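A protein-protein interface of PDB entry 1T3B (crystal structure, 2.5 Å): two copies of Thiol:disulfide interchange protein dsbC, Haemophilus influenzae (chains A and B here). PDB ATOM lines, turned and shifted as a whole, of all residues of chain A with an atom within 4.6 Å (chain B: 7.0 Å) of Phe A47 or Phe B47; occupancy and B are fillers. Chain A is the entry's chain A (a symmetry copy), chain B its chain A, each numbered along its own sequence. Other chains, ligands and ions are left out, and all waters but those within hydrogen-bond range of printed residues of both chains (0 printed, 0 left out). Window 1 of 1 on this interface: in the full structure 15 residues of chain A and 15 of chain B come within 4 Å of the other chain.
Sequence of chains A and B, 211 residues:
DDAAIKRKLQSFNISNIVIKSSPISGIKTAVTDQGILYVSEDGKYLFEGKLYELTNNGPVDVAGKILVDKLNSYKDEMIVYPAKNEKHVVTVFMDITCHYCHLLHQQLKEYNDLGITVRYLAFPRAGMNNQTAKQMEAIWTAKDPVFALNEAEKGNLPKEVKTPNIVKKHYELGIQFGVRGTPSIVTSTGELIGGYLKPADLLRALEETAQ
Of the 10 printed residues of chain A, 7 touch a printed residue of chain B.
Printed residues of chain A that touch a printed residue of chain B: Tyr A45, Leu A46, Phe A47, Glu A48, Gly A49, Lys A50 and Leu A51.
Hydrophobic or aromatic side chains of chain A within 4 Å of the printed part of chain B: Tyr A45, Phe A47 and Leu A51.
Among the printed residues, 20 pairs touch across the chains.
Of chain B, only Phe B47, Lys B50 and Leu B51 come within 4 Å of Phe A47.
Ile B27 touches none of the printed residues of chain A.
Printed residues of chain A within 4 Å of Leu B46: Lys A50 (3.9 Å) and Leu A51 (3.3 Å).
Printed residues of chain A within 4 Å of Lys B50: Leu A46, Phe A47, Glu A48 and Gly A49.
The nearest printed residue of chain A that does not touch Tyr B52 is Phe A47 (5.0 Å).
CD1 of Tyr A45 touches CG1 of Ile B24, 3.3 Å away.
Tyr A45 touches Leu B51.
CD1 of Leu B51 touches O of Leu A46, 3.3 Å away.
Phe A47 touches Phe B47.
CA of Phe A47 touches O of Lys B50, 3.9 Å away.
Glu A48 touches Tyr B52.
Lys B50 touches Gly A49 (N to CA, 3.7 Å).
N of Lys A50 touches CA of Gly B49 (3.7 Å).
CD1 of Leu A51 touches O of Leu B46, at 3.3 Å.
Phe B47 touches Leu A51.
O of Tyr B38 lies within hydrogen-bond range of N of Phe B47 (2.9 Å).
N of Ser B40 is in hydrogen-bond range of O of Tyr B45 (3.4 Å).
The backbone NH (N) of Phe A47 is in hydrogen-bond range of the backbone carbonyl oxygen (O) of Tyr A38, 2.9 Å away.
Tyr A45 touches Leu B51, and with the chains exchanged Leu A51 touches Tyr B45.
Leu A46 touches Lys B50, and with the chains exchanged Lys A50 touches Leu B46.
Phe A47 touches Lys B50, and with the chains exchanged Lys A50 touches Phe B47.
Phe A47 touches Leu B51, and with the chains exchanged Leu A51 touches Phe B47.
Positions printed for both chains: 27, 37, 38, 45, 46, 47, 48, 49, 50 and 51.
Of the 20 pairs that touch across the chains among the printed residues, 16 have their exchanged pair printed and touching as well.
N of Glu B48 lies within hydrogen-bond range of O of Lys A50 (3.3 Å).
O of Leu A46 lies within hydrogen-bond range of N of Tyr B52, 2.9 Å away.
O of Lys B50 sits at hydrogen-bond distance from N of Glu A48 (3.3 Å).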
ATOM      1  N   ILE A  27       9.388 -12.322 -15.048  1.00  0.00           N
ATOM      2  CA  ILE A  27       9.445 -11.450 -13.873  1.00  0.00           C
ATOM      3  C   ILE A  27      10.749 -11.612 -13.092  1.00  0.00           C
ATOM      4  O   ILE A  27      11.477 -12.592 -13.259  1.00  0.00           O
ATOM      5  CB  ILE A  27       8.261 -11.738 -12.910  1.00  0.00           C
ATOM      6  CG1 ILE A  27       6.937 -11.641 -13.668  1.00  0.00           C
ATOM      7  CG2 ILE A  27       8.254 -10.737 -11.756  1.00  0.00           C
ATOM      8  CD1 ILE A  27       6.694 -10.278 -14.287  1.00  0.00           C
ATOM      9  N   LEU A  37       9.219  -6.784  -4.106  1.00  0.00           N
ATOM     10  CA  LEU A  37       8.316  -6.640  -5.242  1.00  0.00           C
ATOM     11  C   LEU A  37       8.560  -7.711  -6.294  1.00  0.00           C
ATOM     12  O   LEU A  37       9.381  -8.605  -6.114  1.00  0.00           O
ATOM     13  CB  LEU A  37       8.498  -5.266  -5.896  1.00  0.00           C
ATOM     14  CG  LEU A  37       8.368  -4.085  -4.940  1.00  0.00           C
ATOM     15  CD1 LEU A  37       8.482  -2.776  -5.706  1.00  0.00           C
ATOM     16  CD2 LEU A  37       7.045  -4.173  -4.215  1.00  0.00           C
ATOM     17  N   TYR A  38       7.827  -7.605  -7.395  1.00  0.00           N
ATOM     18  CA  TYR A  38       7.957  -8.535  -8.504  1.00  0.00           C
ATOM     19  C   TYR A  38       7.689  -7.745  -9.768  1.00  0.00           C
ATOM     20  O   TYR A  38       6.627  -7.148  -9.923  1.00  0.00           O
ATOM     21  CB  TYR A  38       6.966  -9.676  -8.339  1.00  0.00           C
ATOM     22  CG  TYR A  38       7.345 -10.613  -7.214  1.00  0.00           C
ATOM     23  CD1 TYR A  38       8.223 -11.667  -7.432  1.00  0.00           C
ATOM     24  CD2 TYR A  38       6.858 -10.420  -5.918  1.00  0.00           C
ATOM     25  CE1 TYR A  38       8.609 -12.507  -6.393  1.00  0.00           C
ATOM     26  CE2 TYR A  38       7.239 -11.255  -4.872  1.00  0.00           C
ATOM     27  CZ  TYR A  38       8.117 -12.298  -5.116  1.00  0.00           C
ATOM     28  OH  TYR A  38       8.515 -13.126  -4.085  1.00  0.00           O
ATOM     29  N   TYR A  45       4.855  -3.694 -15.503  1.00  0.00           N
ATOM     30  CA  TYR A  45       3.943  -4.248 -14.515  1.00  0.00           C
ATOM     31  C   TYR A  45       4.628  -4.588 -13.194  1.00  0.00           C
ATOM     32  O   TYR A  45       5.601  -5.360 -13.167  1.00  0.00           O
ATOM     33  CB  TYR A  45       3.293  -5.506 -15.092  1.00  0.00           C
ATOM     34  CG  TYR A  45       2.323  -5.237 -16.218  1.00  0.00           C
ATOM     35  CD1 TYR A  45       2.089  -6.198 -17.201  1.00  0.00           C
ATOM     36  CD2 TYR A  45       1.584  -4.049 -16.263  1.00  0.00           C
ATOM     37  CE1 TYR A  45       1.141  -5.987 -18.196  1.00  0.00           C
ATOM     38  CE2 TYR A  45       0.631  -3.831 -17.254  1.00  0.00           C
ATOM     39  CZ  TYR A  45       0.411  -4.802 -18.214  1.00  0.00           C
ATOM     40  OH  TYR A  45      -0.573  -4.596 -19.156  1.00  0.00           O
ATOM     41  N   LEU A  46       4.098  -4.025 -12.105  1.00  0.00           N
ATOM     42  CA  LEU A  46       4.637  -4.257 -10.770  1.00  0.00           C
ATOM     43  C   LEU A  46       3.662  -4.959  -9.825  1.00  0.00           C
ATOM     44  O   LEU A  46       2.485  -4.617  -9.767  1.00  0.00           O
ATOM     45  CB  LEU A  46       5.035  -2.937 -10.119  1.00  0.00           C
ATOM     46  CG  LEU A  46       5.442  -3.129  -8.654  1.00  0.00           C
ATOM     47  CD1 LEU A  46       6.886  -3.597  -8.616  1.00  0.00           C
ATOM     48  CD2 LEU A  46       5.253  -1.844  -7.857  1.00  0.00           C
ATOM     49  N   PHE A  47       4.159  -5.937  -9.076  1.00  0.00           N
ATOM     50  CA  PHE A  47       3.330  -6.623  -8.094  1.00  0.00           C
ATOM     51  C   PHE A  47       3.745  -6.095  -6.746  1.00  0.00           C
ATOM     52  O   PHE A  47       4.854  -6.380  -6.280  1.00  0.00           O
ATOM     53  CB  PHE A  47       3.569  -8.119  -8.093  1.00  0.00           C
ATOM     54  CG  PHE A  47       3.123  -8.791  -9.334  1.00  0.00           C
ATOM     55  CD1 PHE A  47       3.855  -8.670 -10.511  1.00  0.00           C
ATOM     56  CD2 PHE A  47       1.962  -9.547  -9.337  1.00  0.00           C
ATOM     57  CE1 PHE A  47       3.431  -9.300 -11.681  1.00  0.00           C
ATOM     58  CE2 PHE A  47       1.527 -10.180 -10.493  1.00  0.00           C
ATOM     59  CZ  PHE A  47       2.264 -10.057 -11.671  1.00  0.00           C
ATOM     60  N   GLU A  48       2.873  -5.311  -6.129  1.00  0.00           N
ATOM     61  CA  GLU A  48       3.158  -4.760  -4.818  1.00  0.00           C
ATOM     62  C   GLU A  48       2.405  -5.658  -3.855  1.00  0.00           C
ATOM     63  O   GLU A  48       1.857  -5.205  -2.860  1.00  0.00           O
ATOM     64  CB  GLU A  48       2.675  -3.304  -4.739  1.00  0.00           C
ATOM     65  CG  GLU A  48       3.059  -2.561  -3.461  1.00  0.00           C
ATOM     66  CD  GLU A  48       3.490  -1.120  -3.727  1.00  0.00           C
ATOM     67  OE1 GLU A  48       2.752  -0.398  -4.443  1.00  0.00           O
ATOM     68  OE2 GLU A  48       4.562  -0.713  -3.215  1.00  0.00           O
ATOM     69  N   GLY A  49       2.371  -6.945  -4.182  1.00  0.00           N
ATOM     70  CA  GLY A  49       1.689  -7.911  -3.343  1.00  0.00           C
ATOM     71  C   GLY A  49       2.644  -8.871  -2.646  1.00  0.00           C
ATOM     72  O   GLY A  49       3.674  -8.457  -2.104  1.00  0.00           O
ATOM     73  N   LYS A  50       2.305 -10.160  -2.682  1.00  0.00           N
ATOM     74  CA  LYS A  50       3.105 -11.203  -2.044  1.00  0.00           C
ATOM     75  C   LYS A  50       2.945 -12.557  -2.778  1.00  0.00           C
ATOM     76  O   LYS A  50       1.865 -13.157  -2.772  1.00  0.00           O
ATOM     77  CB  LYS A  50       2.668 -11.316  -0.576  1.00  0.00           C
ATOM     78  CG  LYS A  50       3.396 -12.362   0.224  1.00  0.00           C
ATOM     79  CD  LYS A  50       2.925 -12.414   1.674  1.00  0.00           C
ATOM     80  CE  LYS A  50       3.617 -11.384   2.566  1.00  0.00           C
ATOM     81  NZ  LYS A  50       3.276 -11.595   4.015  1.00  0.00           N
ATOM     82  N   LEU A  51       4.024 -13.036  -3.403  1.00  0.00           N
ATOM     83  CA  LEU A  51       3.991 -14.296  -4.158  1.00  0.00           C
ATOM     84  C   LEU A  51       4.289 -15.580  -3.366  1.00  0.00           C
ATOM     85  O   LEU A  51       5.310 -15.682  -2.689  1.00  0.00           O
ATOM     86  CB  LEU A  51       4.948 -14.205  -5.352  1.00  0.00           C
ATOM     87  CG  LEU A  51       5.204 -15.503  -6.135  1.00  0.00           C
ATOM     88  CD1 LEU A  51       3.894 -16.083  -6.656  1.00  0.00           C
ATOM     89  CD2 LEU A  51       6.164 -15.219  -7.282  1.00  0.00           C
ATOM     90  N   ILE B  24      -0.163 -10.277 -17.989  1.00  0.00           N
ATOM     91  CA  ILE B  24       1.128 -10.947 -17.879  1.00  0.00           C
ATOM     92  C   ILE B  24       0.989 -12.433 -18.220  1.00  0.00           C
ATOM     93  O   ILE B  24       0.364 -13.220 -17.484  1.00  0.00           O
ATOM     94  CB  ILE B  24       1.734 -10.788 -16.455  1.00  0.00           C
ATOM     95  CG1 ILE B  24       2.181  -9.333 -16.237  1.00  0.00           C
ATOM     96  CG2 ILE B  24       2.919 -11.720 -16.289  1.00  0.00           C
ATOM     97  N   ILE B  27       0.664 -16.252 -16.645  1.00  0.00           N
ATOM     98  CA  ILE B  27      -0.280 -16.083 -15.537  1.00  0.00           C
ATOM     99  C   ILE B  27      -1.699 -15.786 -16.023  1.00  0.00           C
ATOM    100  O   ILE B  27      -1.913 -15.408 -17.176  1.00  0.00           O
ATOM    101  CB  ILE B  27       0.167 -14.928 -14.599  1.00  0.00           C
ATOM    102  CG1 ILE B  27       1.605 -15.160 -14.135  1.00  0.00           C
ATOM    103  CG2 ILE B  27      -0.749 -14.847 -13.379  1.00  0.00           C
ATOM    104  CD1 ILE B  27       1.792 -16.457 -13.373  1.00  0.00           C
ATOM    105  N   ILE B  36      -9.113 -10.838  -6.398  1.00  0.00           N
ATOM    106  CA  ILE B  36      -8.545 -10.929  -7.728  1.00  0.00           C
ATOM    107  C   ILE B  36      -7.083 -11.384  -7.625  1.00  0.00           C
ATOM    108  O   ILE B  36      -6.158 -10.575  -7.491  1.00  0.00           O
ATOM    109  CB  ILE B  36      -8.680  -9.563  -8.464  1.00  0.00           C
ATOM    110  CG1 ILE B  36     -10.160  -9.325  -8.794  1.00  0.00           C
ATOM    111  CG2 ILE B  36      -7.823  -9.531  -9.736  1.00  0.00           C
ATOM    112  CD1 ILE B  36     -10.458  -7.978  -9.423  1.00  0.00           C
ATOM    113  N   LEU B  37      -6.904 -12.705  -7.668  1.00  0.00           N
ATOM    114  CA  LEU B  37      -5.590 -13.333  -7.592  1.00  0.00           C
ATOM    115  C   LEU B  37      -4.898 -13.359  -8.946  1.00  0.00           C
ATOM    116  O   LEU B  37      -5.407 -12.832  -9.931  1.00  0.00           O
ATOM    117  CB  LEU B  37      -5.715 -14.772  -7.082  1.00  0.00           C
ATOM    118  CG  LEU B  37      -6.469 -14.916  -5.764  1.00  0.00           C
ATOM    119  CD1 LEU B  37      -6.462 -16.368  -5.311  1.00  0.00           C
ATOM    120  CD2 LEU B  37      -5.831 -14.023  -4.724  1.00  0.00           C
ATOM    121  N   TYR B  38      -3.727 -13.980  -8.975  1.00  0.00           N
ATOM    122  CA  TYR B  38      -2.952 -14.113 -10.197  1.00  0.00           C
ATOM    123  C   TYR B  38      -2.227 -15.441 -10.110  1.00  0.00           C
ATOM    124  O   TYR B  38      -1.468 -15.682  -9.175  1.00  0.00           O
ATOM    125  CB  TYR B  38      -1.978 -12.953 -10.318  1.00  0.00           C
ATOM    126  CG  TYR B  38      -2.671 -11.646 -10.633  1.00  0.00           C
ATOM    127  CD1 TYR B  38      -2.954 -11.290 -11.945  1.00  0.00           C
ATOM    128  CD2 TYR B  38      -3.083 -10.783  -9.614  1.00  0.00           C
ATOM    129  CE1 TYR B  38      -3.629 -10.111 -12.240  1.00  0.00           C
ATOM    130  CE2 TYR B  38      -3.760  -9.601  -9.899  1.00  0.00           C
ATOM    131  CZ  TYR B  38      -4.032  -9.270 -11.216  1.00  0.00           C
ATOM    132  OH  TYR B  38      -4.715  -8.107 -11.513  1.00  0.00           O
ATOM    133  N   VAL B  39      -2.473 -16.305 -11.089  1.00  0.00           N
ATOM    134  CA  VAL B  39      -1.885 -17.639 -11.087  1.00  0.00           C
ATOM    135  C   VAL B  39      -1.142 -18.027 -12.361  1.00  0.00           C
ATOM    136  O   VAL B  39      -1.436 -17.540 -13.455  1.00  0.00           O
ATOM    137  CB  VAL B  39      -2.977 -18.704 -10.814  1.00  0.00           C
ATOM    138  CG1 VAL B  39      -2.370 -20.102 -10.802  1.00  0.00           C
ATOM    139  CG2 VAL B  39      -3.662 -18.405  -9.490  1.00  0.00           C
ATOM    140  N   SER B  40      -0.189 -18.937 -12.193  1.00  0.00           N
ATOM    141  CA  SER B  40       0.632 -19.428 -13.288  1.00  0.00           C
ATOM    142  C   SER B  40      -0.114 -20.397 -14.198  1.00  0.00           C
ATOM    143  O   SER B  40      -0.981 -21.147 -13.745  1.00  0.00           O
ATOM    144  CB  SER B  40       1.879 -20.106 -12.722  1.00  0.00           C
ATOM    145  N   TYR B  45       2.201 -21.362  -8.476  1.00  0.00           N
ATOM    146  CA  TYR B  45       2.490 -20.076  -7.860  1.00  0.00           C
ATOM    147  C   TYR B  45       1.291 -19.132  -7.857  1.00  0.00           C
ATOM    148  O   TYR B  45       0.720 -18.833  -8.918  1.00  0.00           O
ATOM    149  CB  TYR B  45       3.653 -19.422  -8.606  1.00  0.00           C
ATOM    150  CG  TYR B  45       4.981 -20.111  -8.402  1.00  0.00           C
ATOM    151  CD1 TYR B  45       5.976 -20.044  -9.376  1.00  0.00           C
ATOM    152  CD2 TYR B  45       5.272 -20.773  -7.203  1.00  0.00           C
ATOM    153  CE1 TYR B  45       7.227 -20.610  -9.162  1.00  0.00           C
ATOM    154  CE2 TYR B  45       6.523 -21.341  -6.979  1.00  0.00           C
ATOM    155  CZ  TYR B  45       7.497 -21.254  -7.958  1.00  0.00           C
ATOM    156  OH  TYR B  45       8.746 -21.773  -7.701  1.00  0.00           O
ATOM    157  N   LEU B  46       0.933 -18.654  -6.662  1.00  0.00           N
ATOM    158  CA  LEU B  46      -0.189 -17.737  -6.496  1.00  0.00           C
ATOM    159  C   LEU B  46       0.212 -16.362  -5.964  1.00  0.00           C
ATOM    160  O   LEU B  46       1.006 -16.253  -5.035  1.00  0.00           O
ATOM    161  CB  LEU B  46      -1.215 -18.320  -5.531  1.00  0.00           C
ATOM    162  CG  LEU B  46      -2.318 -17.310  -5.201  1.00  0.00           C
ATOM    163  CD1 LEU B  46      -3.342 -17.336  -6.323  1.00  0.00           C
ATOM    164  CD2 LEU B  46      -2.963 -17.617  -3.855  1.00  0.00           C
ATOM    165  N   PHE B  47      -0.347 -15.310  -6.551  1.00  0.00           N
ATOM    166  CA  PHE B  47      -0.085 -13.959  -6.075  1.00  0.00           C
ATOM    167  C   PHE B  47      -1.316 -13.528  -5.322  1.00  0.00           C
ATOM    168  O   PHE B  47      -2.371 -13.307  -5.927  1.00  0.00           O
ATOM    169  CB  PHE B  47       0.119 -12.983  -7.215  1.00  0.00           C
ATOM    170  CG  PHE B  47       1.350 -13.233  -7.997  1.00  0.00           C
ATOM    171  CD1 PHE B  47       1.422 -14.297  -8.889  1.00  0.00           C
ATOM    172  CD2 PHE B  47       2.452 -12.407  -7.842  1.00  0.00           C
ATOM    173  CE1 PHE B  47       2.585 -14.535  -9.622  1.00  0.00           C
ATOM    174  CE2 PHE B  47       3.617 -12.631  -8.563  1.00  0.00           C
ATOM    175  CZ  PHE B  47       3.685 -13.699  -9.458  1.00  0.00           C
ATOM    176  N   GLU B  48      -1.195 -13.431  -4.005  1.00  0.00           N
ATOM    177  CA  GLU B  48      -2.310 -13.008  -3.180  1.00  0.00           C
ATOM    178  C   GLU B  48      -2.040 -11.541  -2.898  1.00  0.00           C
ATOM    179  O   GLU B  48      -2.301 -11.045  -1.812  1.00  0.00           O
ATOM    180  CB  GLU B  48      -2.359 -13.838  -1.890  1.00  0.00           C
ATOM    181  CG  GLU B  48      -3.582 -13.597  -1.008  1.00  0.00           C
ATOM    182  CD  GLU B  48      -4.141 -14.887  -0.412  1.00  0.00           C
ATOM    183  OE1 GLU B  48      -3.345 -15.676   0.157  1.00  0.00           O
ATOM    184  OE2 GLU B  48      -5.373 -15.106  -0.510  1.00  0.00           O
ATOM    185  N   GLY B  49      -1.491 -10.859  -3.897  1.00  0.00           N
ATOM    186  CA  GLY B  49      -1.188  -9.448  -3.760  1.00  0.00           C
ATOM    187  C   GLY B  49      -2.080  -8.563  -4.621  1.00  0.00           C
ATOM    188  O   GLY B  49      -3.299  -8.755  -4.677  1.00  0.00           O
ATOM    189  N   LYS B  50      -1.460  -7.605  -5.310  1.00  0.00           N
ATOM    190  CA  LYS B  50      -2.174  -6.661  -6.167  1.00  0.00           C
ATOM    191  C   LYS B  50      -1.278  -6.173  -7.330  1.00  0.00           C
ATOM    192  O   LYS B  50      -0.284  -5.470  -7.112  1.00  0.00           O
ATOM    193  CB  LYS B  50      -2.644  -5.483  -5.300  1.00  0.00           C
ATOM    194  CG  LYS B  50      -3.395  -4.410  -6.041  1.00  0.00           C
ATOM    195  CD  LYS B  50      -3.844  -3.278  -5.122  1.00  0.00           C
ATOM    196  CE  LYS B  50      -5.161  -3.574  -4.405  1.00  0.00           C
ATOM    197  NZ  LYS B  50      -5.669  -2.367  -3.669  1.00  0.00           N
ATOM    198  N   LEU B  51      -1.634  -6.541  -8.563  1.00  0.00           N
ATOM    199  CA  LEU B  51      -0.849  -6.164  -9.746  1.00  0.00           C
ATOM    200  C   LEU B  51      -1.199  -4.820 -10.405  1.00  0.00           C
ATOM    201  O   LEU B  51      -2.353  -4.561 -10.738  1.00  0.00           O
ATOM    202  CB  LEU B  51      -0.934  -7.279 -10.796  1.00  0.00           C
ATOM    203  CG  LEU B  51      -0.348  -6.971 -12.183  1.00  0.00           C
ATOM    204  CD1 LEU B  51       1.121  -6.577 -12.069  1.00  0.00           C
ATOM    205  CD2 LEU B  51      -0.513  -8.188 -13.082  1.00  0.00           C
ATOM    206  N   TYR B  52      -0.184  -3.985 -10.618  1.00  0.00           N
ATOM    207  CA  TYR B  52      -0.375  -2.671 -11.222  1.00  0.00           C
ATOM    208  C   TYR B  52       0.283  -2.471 -12.586  1.00  0.00           C
ATOM    209  O   TYR B  52       0.594  -3.411 -13.321  1.00  0.00           O
ATOM    210  CB  TYR B  52       0.193  -1.577 -10.324  1.00  0.00           C
ATOM    211  CG  TYR B  52      -0.399  -1.454  -8.953  1.00  0.00           C
ATOM    212  CD1 TYR B  52      -0.114  -2.386  -7.956  1.00  0.00           C
ATOM    213  CD2 TYR B  52      -1.202  -0.361  -8.628  1.00  0.00           C
ATOM    214  CE1 TYR B  52      -0.612  -2.226  -6.654  1.00  0.00           C
ATOM    215  CE2 TYR B  52      -1.707  -0.193  -7.333  1.00  0.00           C
ATOM    216  CZ  TYR B  52      -1.408  -1.124  -6.352  1.00  0.00           C
ATOM    217  OH  TYR B  52      -1.897  -0.934  -5.080  1.00  0.00           O
